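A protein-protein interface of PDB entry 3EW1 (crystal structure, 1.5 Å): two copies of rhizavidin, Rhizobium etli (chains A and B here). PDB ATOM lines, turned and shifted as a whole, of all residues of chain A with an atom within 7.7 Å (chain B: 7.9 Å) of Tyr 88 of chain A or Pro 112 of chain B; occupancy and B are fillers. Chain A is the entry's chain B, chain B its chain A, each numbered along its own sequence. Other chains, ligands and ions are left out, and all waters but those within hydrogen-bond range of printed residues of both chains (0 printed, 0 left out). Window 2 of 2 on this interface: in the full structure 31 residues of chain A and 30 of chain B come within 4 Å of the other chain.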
ATOM      1  N   ASN A  62     -20.449  -7.626 -24.397  1.00  0.00           N
ATOM      2  CA  ASN A  62     -21.185  -6.815 -25.363  1.00  0.00           C
ATOM      3  C   ASN A  62     -21.868  -7.798 -26.285  1.00  0.00           C
ATOM      4  O   ASN A  62     -21.207  -8.419 -27.090  1.00  0.00           O
ATOM      5  CB  ASN A  62     -20.238  -5.900 -26.147  1.00  0.00           C
ATOM      6  CG  ASN A  62     -20.954  -5.062 -27.228  1.00  0.00           C
ATOM      7  OD1 ASN A  62     -22.186  -4.992 -27.288  1.00  0.00           O
ATOM      8  ND2 ASN A  62     -20.196  -4.411 -28.044  1.00  0.00           N
ATOM      9  N   GLY A  63     -23.169  -7.932 -26.136  1.00  0.00           N
ATOM     10  CA  GLY A  63     -23.892  -8.891 -27.006  1.00  0.00           C
ATOM     11  C   GLY A  63     -23.484 -10.313 -26.638  1.00  0.00           C
ATOM     12  O   GLY A  63     -23.532 -10.677 -25.471  1.00  0.00           O
ATOM     13  N   THR A  64     -23.028 -11.101 -27.616  1.00  0.00           N
ATOM     14  CA  THR A  64     -22.513 -12.432 -27.320  1.00  0.00           C
ATOM     15  C   THR A  64     -21.018 -12.442 -27.060  1.00  0.00           C
ATOM     16  O   THR A  64     -20.429 -13.495 -26.819  1.00  0.00           O
ATOM     17  CB  THR A  64     -22.766 -13.418 -28.484  1.00  0.00           C
ATOM     18  OG1 THR A  64     -22.186 -12.904 -29.689  1.00  0.00           O
ATOM     19  CG2 THR A  64     -24.252 -13.616 -28.704  1.00  0.00           C
ATOM     20  N   PHE A  65     -20.390 -11.274 -27.168  1.00  0.00           N
ATOM     21  CA  PHE A  65     -18.936 -11.151 -27.009  1.00  0.00           C
ATOM     22  C   PHE A  65     -18.519 -10.855 -25.590  1.00  0.00           C
ATOM     23  O   PHE A  65     -19.236 -10.195 -24.847  1.00  0.00           O
ATOM     24  CB  PHE A  65     -18.426 -10.132 -27.991  1.00  0.00           C
ATOM     25  CG  PHE A  65     -18.678 -10.556 -29.430  1.00  0.00           C
ATOM     26  CD1 PHE A  65     -19.750 -10.042 -30.147  1.00  0.00           C
ATOM     27  CD2 PHE A  65     -17.861 -11.495 -30.042  1.00  0.00           C
ATOM     28  CE1 PHE A  65     -20.000 -10.461 -31.441  1.00  0.00           C
ATOM     29  CE2 PHE A  65     -18.084 -11.909 -31.352  1.00  0.00           C
ATOM     30  CZ  PHE A  65     -19.166 -11.394 -32.060  1.00  0.00           C
ATOM     31  N   ILE A  66     -17.370 -11.409 -25.209  1.00  0.00           N
ATOM     32  CA  ILE A  66     -16.947 -11.303 -23.826  1.00  0.00           C
ATOM     33  C   ILE A  66     -15.451 -11.243 -23.769  1.00  0.00           C
ATOM     34  O   ILE A  66     -14.726 -11.874 -24.537  1.00  0.00           O
ATOM     35  CB  ILE A  66     -17.471 -12.514 -22.963  1.00  0.00           C
ATOM     36  CG1 ILE A  66     -17.118 -12.317 -21.477  1.00  0.00           C
ATOM     37  CG2 ILE A  66     -16.971 -13.859 -23.510  1.00  0.00           C
ATOM     38  CD1 ILE A  66     -17.754 -13.359 -20.523  1.00  0.00           C
ATOM     39  N   ALA A  67     -14.978 -10.458 -22.814  1.00  0.00           N
ATOM     40  CA  ALA A  67     -13.533 -10.436 -22.497  1.00  0.00           C
ATOM     41  C   ALA A  67     -13.410 -10.476 -20.986  1.00  0.00           C
ATOM     42  O   ALA A  67     -14.129  -9.758 -20.274  1.00  0.00           O
ATOM     43  CB  ALA A  67     -12.848  -9.210 -23.107  1.00  0.00           C
ATOM     44  N   PHE A  68     -12.485 -11.290 -20.467  1.00  0.00           N
ATOM     45  CA  PHE A  68     -12.333 -11.363 -19.028  1.00  0.00           C
ATOM     46  C   PHE A  68     -10.874 -11.598 -18.666  1.00  0.00           C
ATOM     47  O   PHE A  68     -10.052 -12.009 -19.504  1.00  0.00           O
ATOM     48  CB  PHE A  68     -13.295 -12.386 -18.390  1.00  0.00           C
ATOM     49  CG  PHE A  68     -13.163 -13.795 -18.903  1.00  0.00           C
ATOM     50  CD1 PHE A  68     -13.870 -14.209 -20.038  1.00  0.00           C
ATOM     51  CD2 PHE A  68     -12.359 -14.712 -18.250  1.00  0.00           C
ATOM     52  CE1 PHE A  68     -13.778 -15.523 -20.498  1.00  0.00           C
ATOM     53  CE2 PHE A  68     -12.272 -16.051 -18.693  1.00  0.00           C
ATOM     54  CZ  PHE A  68     -12.967 -16.432 -19.826  1.00  0.00           C
ATOM     55  N   THR A  86     -10.505 -13.522 -24.558  1.00  0.00           N
ATOM     56  CA  THR A  86     -11.449 -12.769 -25.393  1.00  0.00           C
ATOM     57  C   THR A  86     -12.150 -13.794 -26.278  1.00  0.00           C
ATOM     58  O   THR A  86     -11.486 -14.682 -26.778  1.00  0.00           O
ATOM     59  CB  THR A  86     -10.670 -11.715 -26.244  1.00  0.00           C
ATOM     60  OG1 THR A  86      -9.705 -11.027 -25.422  1.00  0.00           O
ATOM     61  CG2 THR A  86     -11.629 -10.710 -26.853  1.00  0.00           C
ATOM     62  N   GLY A  87     -13.469 -13.672 -26.474  1.00  0.00           N
ATOM     63  CA  GLY A  87     -14.183 -14.609 -27.350  1.00  0.00           C
ATOM     64  C   GLY A  87     -15.662 -14.317 -27.331  1.00  0.00           C
ATOM     65  O   GLY A  87     -16.101 -13.168 -27.185  1.00  0.00           O
ATOM     66  N   TYR A  88     -16.444 -15.369 -27.548  1.00  0.00           N
ATOM     67  CA  TYR A  88     -17.886 -15.207 -27.713  1.00  0.00           C
ATOM     68  C   TYR A  88     -18.633 -16.452 -27.264  1.00  0.00           C
ATOM     69  O   TYR A  88     -18.057 -17.526 -27.206  1.00  0.00           O
ATOM     70  CB  TYR A  88     -18.187 -14.937 -29.190  1.00  0.00           C
ATOM     71  CG  TYR A  88     -17.591 -15.994 -30.133  1.00  0.00           C
ATOM     72  CD1 TYR A  88     -16.289 -15.870 -30.644  1.00  0.00           C
ATOM     73  CD2 TYR A  88     -18.325 -17.149 -30.483  1.00  0.00           C
ATOM     74  CE1 TYR A  88     -15.748 -16.869 -31.489  1.00  0.00           C
ATOM     75  CE2 TYR A  88     -17.797 -18.129 -31.309  1.00  0.00           C
ATOM     76  CZ  TYR A  88     -16.531 -17.984 -31.818  1.00  0.00           C
ATOM     77  OH  TYR A  88     -16.041 -18.955 -32.649  1.00  0.00           O
ATOM     78  N   ALA A  89     -19.894 -16.267 -26.902  1.00  0.00           N
ATOM     79  CA  ALA A  89     -20.817 -17.362 -26.555  1.00  0.00           C
ATOM     80  C   ALA A  89     -21.509 -17.867 -27.813  1.00  0.00           C
ATOM     81  O   ALA A  89     -21.898 -17.063 -28.659  1.00  0.00           O
ATOM     82  CB  ALA A  89     -21.860 -16.883 -25.562  1.00  0.00           C
ATOM     83  N   GLN A  90     -21.653 -19.193 -27.936  1.00  0.00           N
ATOM     84  CA  GLN A  90     -22.503 -19.759 -28.993  1.00  0.00           C
ATOM     85  C   GLN A  90     -23.100 -21.059 -28.478  1.00  0.00           C
ATOM     86  O   GLN A  90     -22.707 -21.564 -27.425  1.00  0.00           O
ATOM     87  CB  GLN A  90     -21.684 -20.036 -30.233  1.00  0.00           C
ATOM     88  CG  GLN A  90     -20.523 -20.985 -30.001  1.00  0.00           C
ATOM     89  CD  GLN A  90     -19.817 -21.355 -31.300  1.00  0.00           C
ATOM     90  OE1 GLN A  90     -19.994 -20.703 -32.355  1.00  0.00           O
ATOM     91  NE2 GLN A  90     -19.016 -22.411 -31.235  1.00  0.00           N
ATOM     92  N   VAL A  91     -24.065 -21.593 -29.221  1.00  0.00           N
ATOM     93  CA  VAL A  91     -24.760 -22.787 -28.802  1.00  0.00           C
ATOM     94  C   VAL A  91     -24.314 -23.940 -29.696  1.00  0.00           C
ATOM     95  O   VAL A  91     -24.156 -23.753 -30.906  1.00  0.00           O
ATOM     96  CB  VAL A  91     -26.285 -22.557 -28.900  1.00  0.00           C
ATOM     97  CG1 VAL A  91     -27.061 -23.841 -28.618  1.00  0.00           C
ATOM     98  CG2 VAL A  91     -26.726 -21.518 -27.910  1.00  0.00           C
ATOM     99  N   THR A  96     -24.695 -24.170 -24.162  1.00  0.00           N
ATOM    100  CA  THR A  96     -23.945 -22.954 -24.436  1.00  0.00           C
ATOM    101  C   THR A  96     -22.440 -23.189 -24.183  1.00  0.00           C
ATOM    102  O   THR A  96     -22.070 -23.920 -23.269  1.00  0.00           O
ATOM    103  CB  THR A  96     -24.424 -21.849 -23.500  1.00  0.00           C
ATOM    104  OG1 THR A  96     -25.861 -21.847 -23.519  1.00  0.00           O
ATOM    105  CG2 THR A  96     -23.931 -20.506 -23.968  1.00  0.00           C
ATOM    106  N   GLU A  97     -21.591 -22.578 -25.001  1.00  0.00           N
ATOM    107  CA  GLU A  97     -20.129 -22.661 -24.801  1.00  0.00           C
ATOM    108  C   GLU A  97     -19.541 -21.283 -25.057  1.00  0.00           C
ATOM    109  O   GLU A  97     -20.137 -20.459 -25.773  1.00  0.00           O
ATOM    110  CB  GLU A  97     -19.456 -23.729 -25.694  1.00  0.00           C
ATOM    111  CG  GLU A  97     -19.596 -23.490 -27.199  1.00  0.00           C
ATOM    112  CD  GLU A  97     -18.935 -24.575 -28.092  1.00  0.00           C
ATOM    113  OE1 GLU A  97     -18.965 -24.382 -29.340  1.00  0.00           O
ATOM    114  OE2 GLU A  97     -18.405 -25.603 -27.571  1.00  0.00           O
ATOM    115  N   ILE A  98     -18.396 -21.006 -24.434  1.00  0.00           N
ATOM    116  CA  ILE A  98     -17.703 -19.762 -24.740  1.00  0.00           C
ATOM    117  C   ILE A  98     -16.392 -20.116 -25.395  1.00  0.00           C
ATOM    118  O   ILE A  98     -15.593 -20.835 -24.812  1.00  0.00           O
ATOM    119  CB  ILE A  98     -17.451 -18.945 -23.453  1.00  0.00           C
ATOM    120  CG1 ILE A  98     -18.778 -18.688 -22.719  1.00  0.00           C
ATOM    121  CG2 ILE A  98     -16.757 -17.603 -23.758  1.00  0.00           C
ATOM    122  CD1 ILE A  98     -18.653 -18.051 -21.298  1.00  0.00           C
ATOM    123  N   VAL A  99     -16.192 -19.645 -26.616  1.00  0.00           N
ATOM    124  CA  VAL A  99     -14.997 -19.926 -27.394  1.00  0.00           C
ATOM    125  C   VAL A  99     -14.076 -18.725 -27.256  1.00  0.00           C
ATOM    126  O   VAL A  99     -14.474 -17.579 -27.543  1.00  0.00           O
ATOM    127  CB  VAL A  99     -15.331 -20.153 -28.897  1.00  0.00           C
ATOM    128  CG1 VAL A  99     -14.043 -20.348 -29.710  1.00  0.00           C
ATOM    129  CG2 VAL A  99     -16.247 -21.375 -29.085  1.00  0.00           C
ATOM    130  N   THR A 100     -12.852 -18.983 -26.791  1.00  0.00           N
ATOM    131  CA  THR A 100     -11.918 -17.892 -26.460  1.00  0.00           C
ATOM    132  C   THR A 100     -10.490 -18.097 -26.978  1.00  0.00           C
ATOM    133  O   THR A 100     -10.053 -19.235 -27.186  1.00  0.00           O
ATOM    134  CB  THR A 100     -11.774 -17.692 -24.918  1.00  0.00           C
ATOM    135  OG1 THR A 100     -11.035 -18.763 -24.340  1.00  0.00           O
ATOM    136  CG2 THR A 100     -13.089 -17.494 -24.195  1.00  0.00           C
ATOM    137  N   SER A 101      -9.773 -16.983 -27.166  1.00  0.00           N
ATOM    138  CA  SER A 101      -8.279 -16.938 -27.259  1.00  0.00           C
ATOM    139  C   SER A 101      -7.815 -16.282 -26.024  1.00  0.00           C
ATOM    140  O   SER A 101      -8.508 -15.398 -25.523  1.00  0.00           O
ATOM    141  CB  SER A 101      -7.844 -16.068 -28.434  1.00  0.00           C
ATOM    142  OG  SER A 101      -8.258 -16.720 -29.650  1.00  0.00           O
ATOM    143  N   ASP A 119      -9.045 -21.538 -25.305  1.00  0.00           N
ATOM    144  CA  ASP A 119      -9.851 -22.312 -24.358  1.00  0.00           C
ATOM    145  C   ASP A 119     -11.288 -22.230 -24.830  1.00  0.00           C
ATOM    146  O   ASP A 119     -11.725 -21.175 -25.269  1.00  0.00           O
ATOM    147  CB  ASP A 119      -9.854 -21.687 -22.962  1.00  0.00           C
ATOM    148  CG  ASP A 119      -8.649 -22.019 -22.146  1.00  0.00           C
ATOM    149  OD1 ASP A 119      -7.788 -22.818 -22.554  1.00  0.00           O
ATOM    150  OD2 ASP A 119      -8.550 -21.438 -21.046  1.00  0.00           O
ATOM    151  N   THR A 120     -12.021 -23.335 -24.691  1.00  0.00           N
ATOM    152  CA  THR A 120     -13.464 -23.343 -24.890  1.00  0.00           C
ATOM    153  C   THR A 120     -14.121 -23.855 -23.623  1.00  0.00           C
ATOM    154  O   THR A 120     -13.814 -24.967 -23.173  1.00  0.00           O
ATOM    155  CB  THR A 120     -13.859 -24.241 -26.100  1.00  0.00           C
ATOM    156  OG1 THR A 120     -13.308 -23.662 -27.278  1.00  0.00           O
ATOM    157  CG2 THR A 120     -15.410 -24.361 -26.261  1.00  0.00           C
ATOM    158  N   PHE A 121     -15.047 -23.055 -23.088  1.00  0.00           N
ATOM    159  CA  PHE A 121     -15.741 -23.325 -21.840  1.00  0.00           C
ATOM    160  C   PHE A 121     -17.138 -23.859 -22.122  1.00  0.00           C
ATOM    161  O   PHE A 121     -17.863 -23.214 -22.855  1.00  0.00           O
ATOM    162  CB  PHE A 121     -15.860 -22.004 -21.036  1.00  0.00           C
ATOM    163  CG  PHE A 121     -14.547 -21.482 -20.529  1.00  0.00           C
ATOM    164  CD1 PHE A 121     -13.732 -20.655 -21.330  1.00  0.00           C
ATOM    165  CD2 PHE A 121     -14.084 -21.858 -19.297  1.00  0.00           C
ATOM    166  CE1 PHE A 121     -12.488 -20.154 -20.854  1.00  0.00           C
ATOM    167  CE2 PHE A 121     -12.829 -21.342 -18.817  1.00  0.00           C
ATOM    168  CZ  PHE A 121     -12.057 -20.541 -19.632  1.00  0.00           C
ATOM    169  N   ALA B  82     -15.704  -7.256 -28.443  1.00  0.00           N
ATOM    170  CA  ALA B  82     -14.954  -7.092 -27.166  1.00  0.00           C
ATOM    171  C   ALA B  82     -13.471  -7.234 -27.390  1.00  0.00           C
ATOM    172  O   ALA B  82     -13.078  -7.988 -28.285  1.00  0.00           O
ATOM    173  CB  ALA B  82     -15.430  -8.090 -26.126  1.00  0.00           C
ATOM    174  N   LEU B 104      -9.237  -9.019 -30.311  1.00  0.00           N
ATOM    175  CA  LEU B 104     -10.526  -8.393 -30.547  1.00  0.00           C
ATOM    176  C   LEU B 104     -11.436  -9.455 -31.090  1.00  0.00           C
ATOM    177  O   LEU B 104     -11.141 -10.034 -32.142  1.00  0.00           O
ATOM    178  CB  LEU B 104     -10.403  -7.254 -31.564  1.00  0.00           C
ATOM    179  CG  LEU B 104     -11.657  -6.732 -32.291  1.00  0.00           C
ATOM    180  CD1 LEU B 104     -12.571  -6.068 -31.268  1.00  0.00           C
ATOM    181  CD2 LEU B 104     -11.256  -5.714 -33.351  1.00  0.00           C
ATOM    182  N   ALA B 105     -12.540  -9.712 -30.394  1.00  0.00           N
ATOM    183  CA  ALA B 105     -13.551 -10.674 -30.889  1.00  0.00           C
ATOM    184  C   ALA B 105     -14.729  -9.871 -31.464  1.00  0.00           C
ATOM    185  O   ALA B 105     -15.240  -8.934 -30.819  1.00  0.00           O
ATOM    186  CB  ALA B 105     -14.041 -11.549 -29.786  1.00  0.00           C
ATOM    187  N   TYR B 106     -15.203 -10.264 -32.654  1.00  0.00           N
ATOM    188  CA  TYR B 106     -16.185  -9.463 -33.372  1.00  0.00           C
ATOM    189  C   TYR B 106     -16.856 -10.355 -34.404  1.00  0.00           C
ATOM    190  O   TYR B 106     -16.408 -11.478 -34.613  1.00  0.00           O
ATOM    191  CB  TYR B 106     -15.512  -8.254 -34.050  1.00  0.00           C
ATOM    192  CG  TYR B 106     -14.564  -8.620 -35.178  1.00  0.00           C
ATOM    193  CD1 TYR B 106     -13.329  -9.249 -34.936  1.00  0.00           C
ATOM    194  CD2 TYR B 106     -14.911  -8.337 -36.495  1.00  0.00           C
ATOM    195  CE1 TYR B 106     -12.477  -9.590 -35.991  1.00  0.00           C
ATOM    196  CE2 TYR B 106     -14.077  -8.671 -37.549  1.00  0.00           C
ATOM    197  CZ  TYR B 106     -12.873  -9.288 -37.299  1.00  0.00           C
ATOM    198  OH  TYR B 106     -12.081  -9.574 -38.378  1.00  0.00           O
ATOM    199  N   GLU B 107     -17.913  -9.824 -35.026  1.00  0.00           N
ATOM    200  CA  GLU B 107     -18.603 -10.484 -36.128  1.00  0.00           C
ATOM    201  C   GLU B 107     -17.904 -10.144 -37.433  1.00  0.00           C
ATOM    202  O   GLU B 107     -17.981  -9.001 -37.899  1.00  0.00           O
ATOM    203  CB  GLU B 107     -20.017  -9.936 -36.224  1.00  0.00           C
ATOM    204  CG  GLU B 107     -21.099 -10.751 -35.549  1.00  0.00           C
ATOM    205  CD  GLU B 107     -20.970 -12.245 -35.794  1.00  0.00           C
ATOM    206  OE1 GLU B 107     -20.642 -12.668 -36.930  1.00  0.00           O
ATOM    207  OE2 GLU B 107     -21.200 -12.994 -34.817  1.00  0.00           O
ATOM    208  N   GLY B 108     -17.240 -11.133 -38.034  1.00  0.00           N
ATOM    209  CA  GLY B 108     -16.520 -10.916 -39.291  1.00  0.00           C
ATOM    210  C   GLY B 108     -17.437 -11.202 -40.472  1.00  0.00           C
ATOM    211  O   GLY B 108     -18.636 -11.466 -40.285  1.00  0.00           O
ATOM    212  N   GLY B 109     -16.864 -11.190 -41.677  1.00  0.00           N
ATOM    213  CA  GLY B 109     -17.628 -11.465 -42.913  1.00  0.00           C
ATOM    214  C   GLY B 109     -18.378 -12.794 -42.913  1.00  0.00           C
ATOM    215  O   GLY B 109     -19.561 -12.862 -43.311  1.00  0.00           O
ATOM    216  N   SER B 110     -17.707 -13.848 -42.443  1.00  0.00           N
ATOM    217  CA  SER B 110     -18.272 -15.206 -42.489  1.00  0.00           C
ATOM    218  C   SER B 110     -18.685 -15.762 -41.132  1.00  0.00           C
ATOM    219  O   SER B 110     -19.188 -16.878 -41.060  1.00  0.00           O
ATOM    220  CB  SER B 110     -17.319 -16.166 -43.205  1.00  0.00           C
ATOM    221  OG  SER B 110     -16.021 -16.108 -42.619  1.00  0.00           O
ATOM    222  N   GLY B 111     -18.492 -14.988 -40.057  1.00  0.00           N
ATOM    223  CA  GLY B 111     -18.931 -15.370 -38.717  1.00  0.00           C
ATOM    224  C   GLY B 111     -17.986 -14.715 -37.688  1.00  0.00           C
ATOM    225  O   GLY B 111     -17.121 -13.934 -38.086  1.00  0.00           O
ATOM    226  N   PRO B 112     -18.153 -15.031 -36.379  1.00  0.00           N
ATOM    227  CA  PRO B 112     -17.252 -14.538 -35.297  1.00  0.00           C
ATOM    228  C   PRO B 112     -15.777 -14.840 -35.599  1.00  0.00           C
ATOM    229  O   PRO B 112     -15.424 -15.945 -36.067  1.00  0.00           O
ATOM    230  CB  PRO B 112     -17.746 -15.282 -34.048  1.00  0.00           C
ATOM    231  CG  PRO B 112     -18.636 -16.395 -34.576  1.00  0.00           C
ATOM    232  CD  PRO B 112     -19.229 -15.869 -35.827  1.00  0.00           C
ATOM    233  N   ALA B 113     -14.932 -13.839 -35.378  1.00  0.00           N
ATOM    234  CA  ALA B 113     -13.518 -13.929 -35.628  1.00  0.00           C
ATOM    235  C   ALA B 113     -12.763 -13.241 -34.472  1.00  0.00           C
ATOM    236  O   ALA B 113     -13.351 -12.465 -33.702  1.00  0.00           O
ATOM    237  CB  ALA B 113     -13.192 -13.272 -36.938  1.00  0.00           C
ATOM    238  N   ILE B 114     -11.473 -13.544 -34.339  1.00  0.00           N
ATOM    239  CA  ILE B 114     -10.628 -12.906 -33.325  1.00  0.00           C
ATOM    240  C   ILE B 114      -9.419 -12.369 -34.058  1.00  0.00           C
ATOM    241  O   ILE B 114      -8.718 -13.136 -34.746  1.00  0.00           O
ATOM    242  CB  ILE B 114     -10.175 -13.885 -32.203  1.00  0.00           C
ATOM    243  CG1 ILE B 114     -11.275 -14.869 -31.790  1.00  0.00           C
ATOM    244  CG2 ILE B 114      -9.653 -13.126 -30.984  1.00  0.00           C
ATOM    245  CD1 ILE B 114     -12.418 -14.290 -31.049  1.00  0.00           C
ATOM    246  N   GLU B 115      -9.216 -11.053 -33.945  1.00  0.00           N
ATOM    247  CA  GLU B 115      -8.125 -10.304 -34.550  1.00  0.00           C
ATOM    248  C   GLU B 115      -7.132 -10.083 -33.409  1.00  0.00           C
ATOM    249  O   GLU B 115      -7.562  -9.839 -32.287  1.00  0.00           O
ATOM    250  CB  GLU B 115      -8.650  -8.939 -35.011  1.00  0.00           C
ATOM    251  CG  GLU B 115      -7.657  -8.005 -35.684  1.00  0.00           C
ATOM    252  CD  GLU B 115      -7.476  -8.307 -37.163  1.00  0.00           C
ATOM    253  OE1 GLU B 115      -6.308  -8.524 -37.582  1.00  0.00           O
ATOM    254  OE2 GLU B 115      -8.502  -8.343 -37.899  1.00  0.00           O
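The backbone NH (N) of Ala 105 of chain B lies within hydrogen-bond range of the backbone carbonyl oxygen (O) of Ala 82 of chain B. N of Ala 113 of chain B lies within hydrogen-bond range of O of Tyr 106 of chain B, at 2.9 Å. O of Ile 66 of chain A is in hydrogen-bond range of N of Gly 87 of chain A (2.9 Å). O of Thr 86 of chain A lies within hydrogen-bond range of N of Ser 101 of chain A, 2.9 Å away. The backbone carbonyl oxygen (O) of Tyr 88 of chain A sits at hydrogen-bond distance from the backbone NH (N) of Val 99 of chain A, 2.9 Å away.
No position is printed for both chains.
Of the 22 printed residues of chain A, 5 touch a printed residue of chain B. Printed residues of chain A that touch a printed residue of chain B: Phe 65, Ile 66, Thr 86, Gly 87 and Tyr 88. Hydrophobic or aromatic side chains of chain A within 4 Å of the printed part of chain B: Phe 65 and Tyr 88. Printed residues of chain B that touch a printed residue of chain A: Ala 82, Ala 105, Tyr 106, Glu 107 and Pro 112. Among the printed residues, no Asp or Glu carboxylate lies within 4 Å of a Lys or Arg side-chain nitrogen of the other chain.
Among the printed residues, pairs that only touch across the chains: Thr 86 of chain A with Ala 82 of chain B (3.4 Å), Phe 65 of chain A with Tyr 106 of chain B (3.5 Å), Phe 65 of chain A with Glu 107 of chain B (3.6 Å), Tyr 88 of chain A with Pro 112 of chain B (3.6 Å), Gly 87 of chain A with Ala 105 of chain B (3.7 Å), Phe 65 of chain A with Ala 105 of chain B (3.7 Å), Thr 86 of chain A with Ala 105 of chain B (3.8 Å), Ile 66 of chain A with Ala 82 of chain B (3.9 Å) and Phe 65 of chain A with Ala 82 of chain B (3.99 Å).
Asn 62 of chain A touches none of the printed residues of chain B. Gly 87 of chain A touches just one residue of chain B: Ala 105. Tyr 88 of chain A touches one residue of chain B. No residue of chain B comes within 4 Å of Ala 89 of chain A. Of the printed residues of chain A, Ala 82 of chain B touches Phe 65, Ile 66 and Thr 86. Of the printed residues of chain A, Tyr 106 of chain B touches Phe 65. Printed residues of chain A within 4 Å of Glu 107 of chain B: Phe 65 (3.6 Å). Pro 112 of chain B touches one residue of chain A. The nearest residue of chain B that does not touch Tyr 88 of chain A is Ile 114 of chain B (4.2 Å). The nearest residue of chain A that does not touch Pro 112 of chain B is Phe 65 of chain A (4.3 Å).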
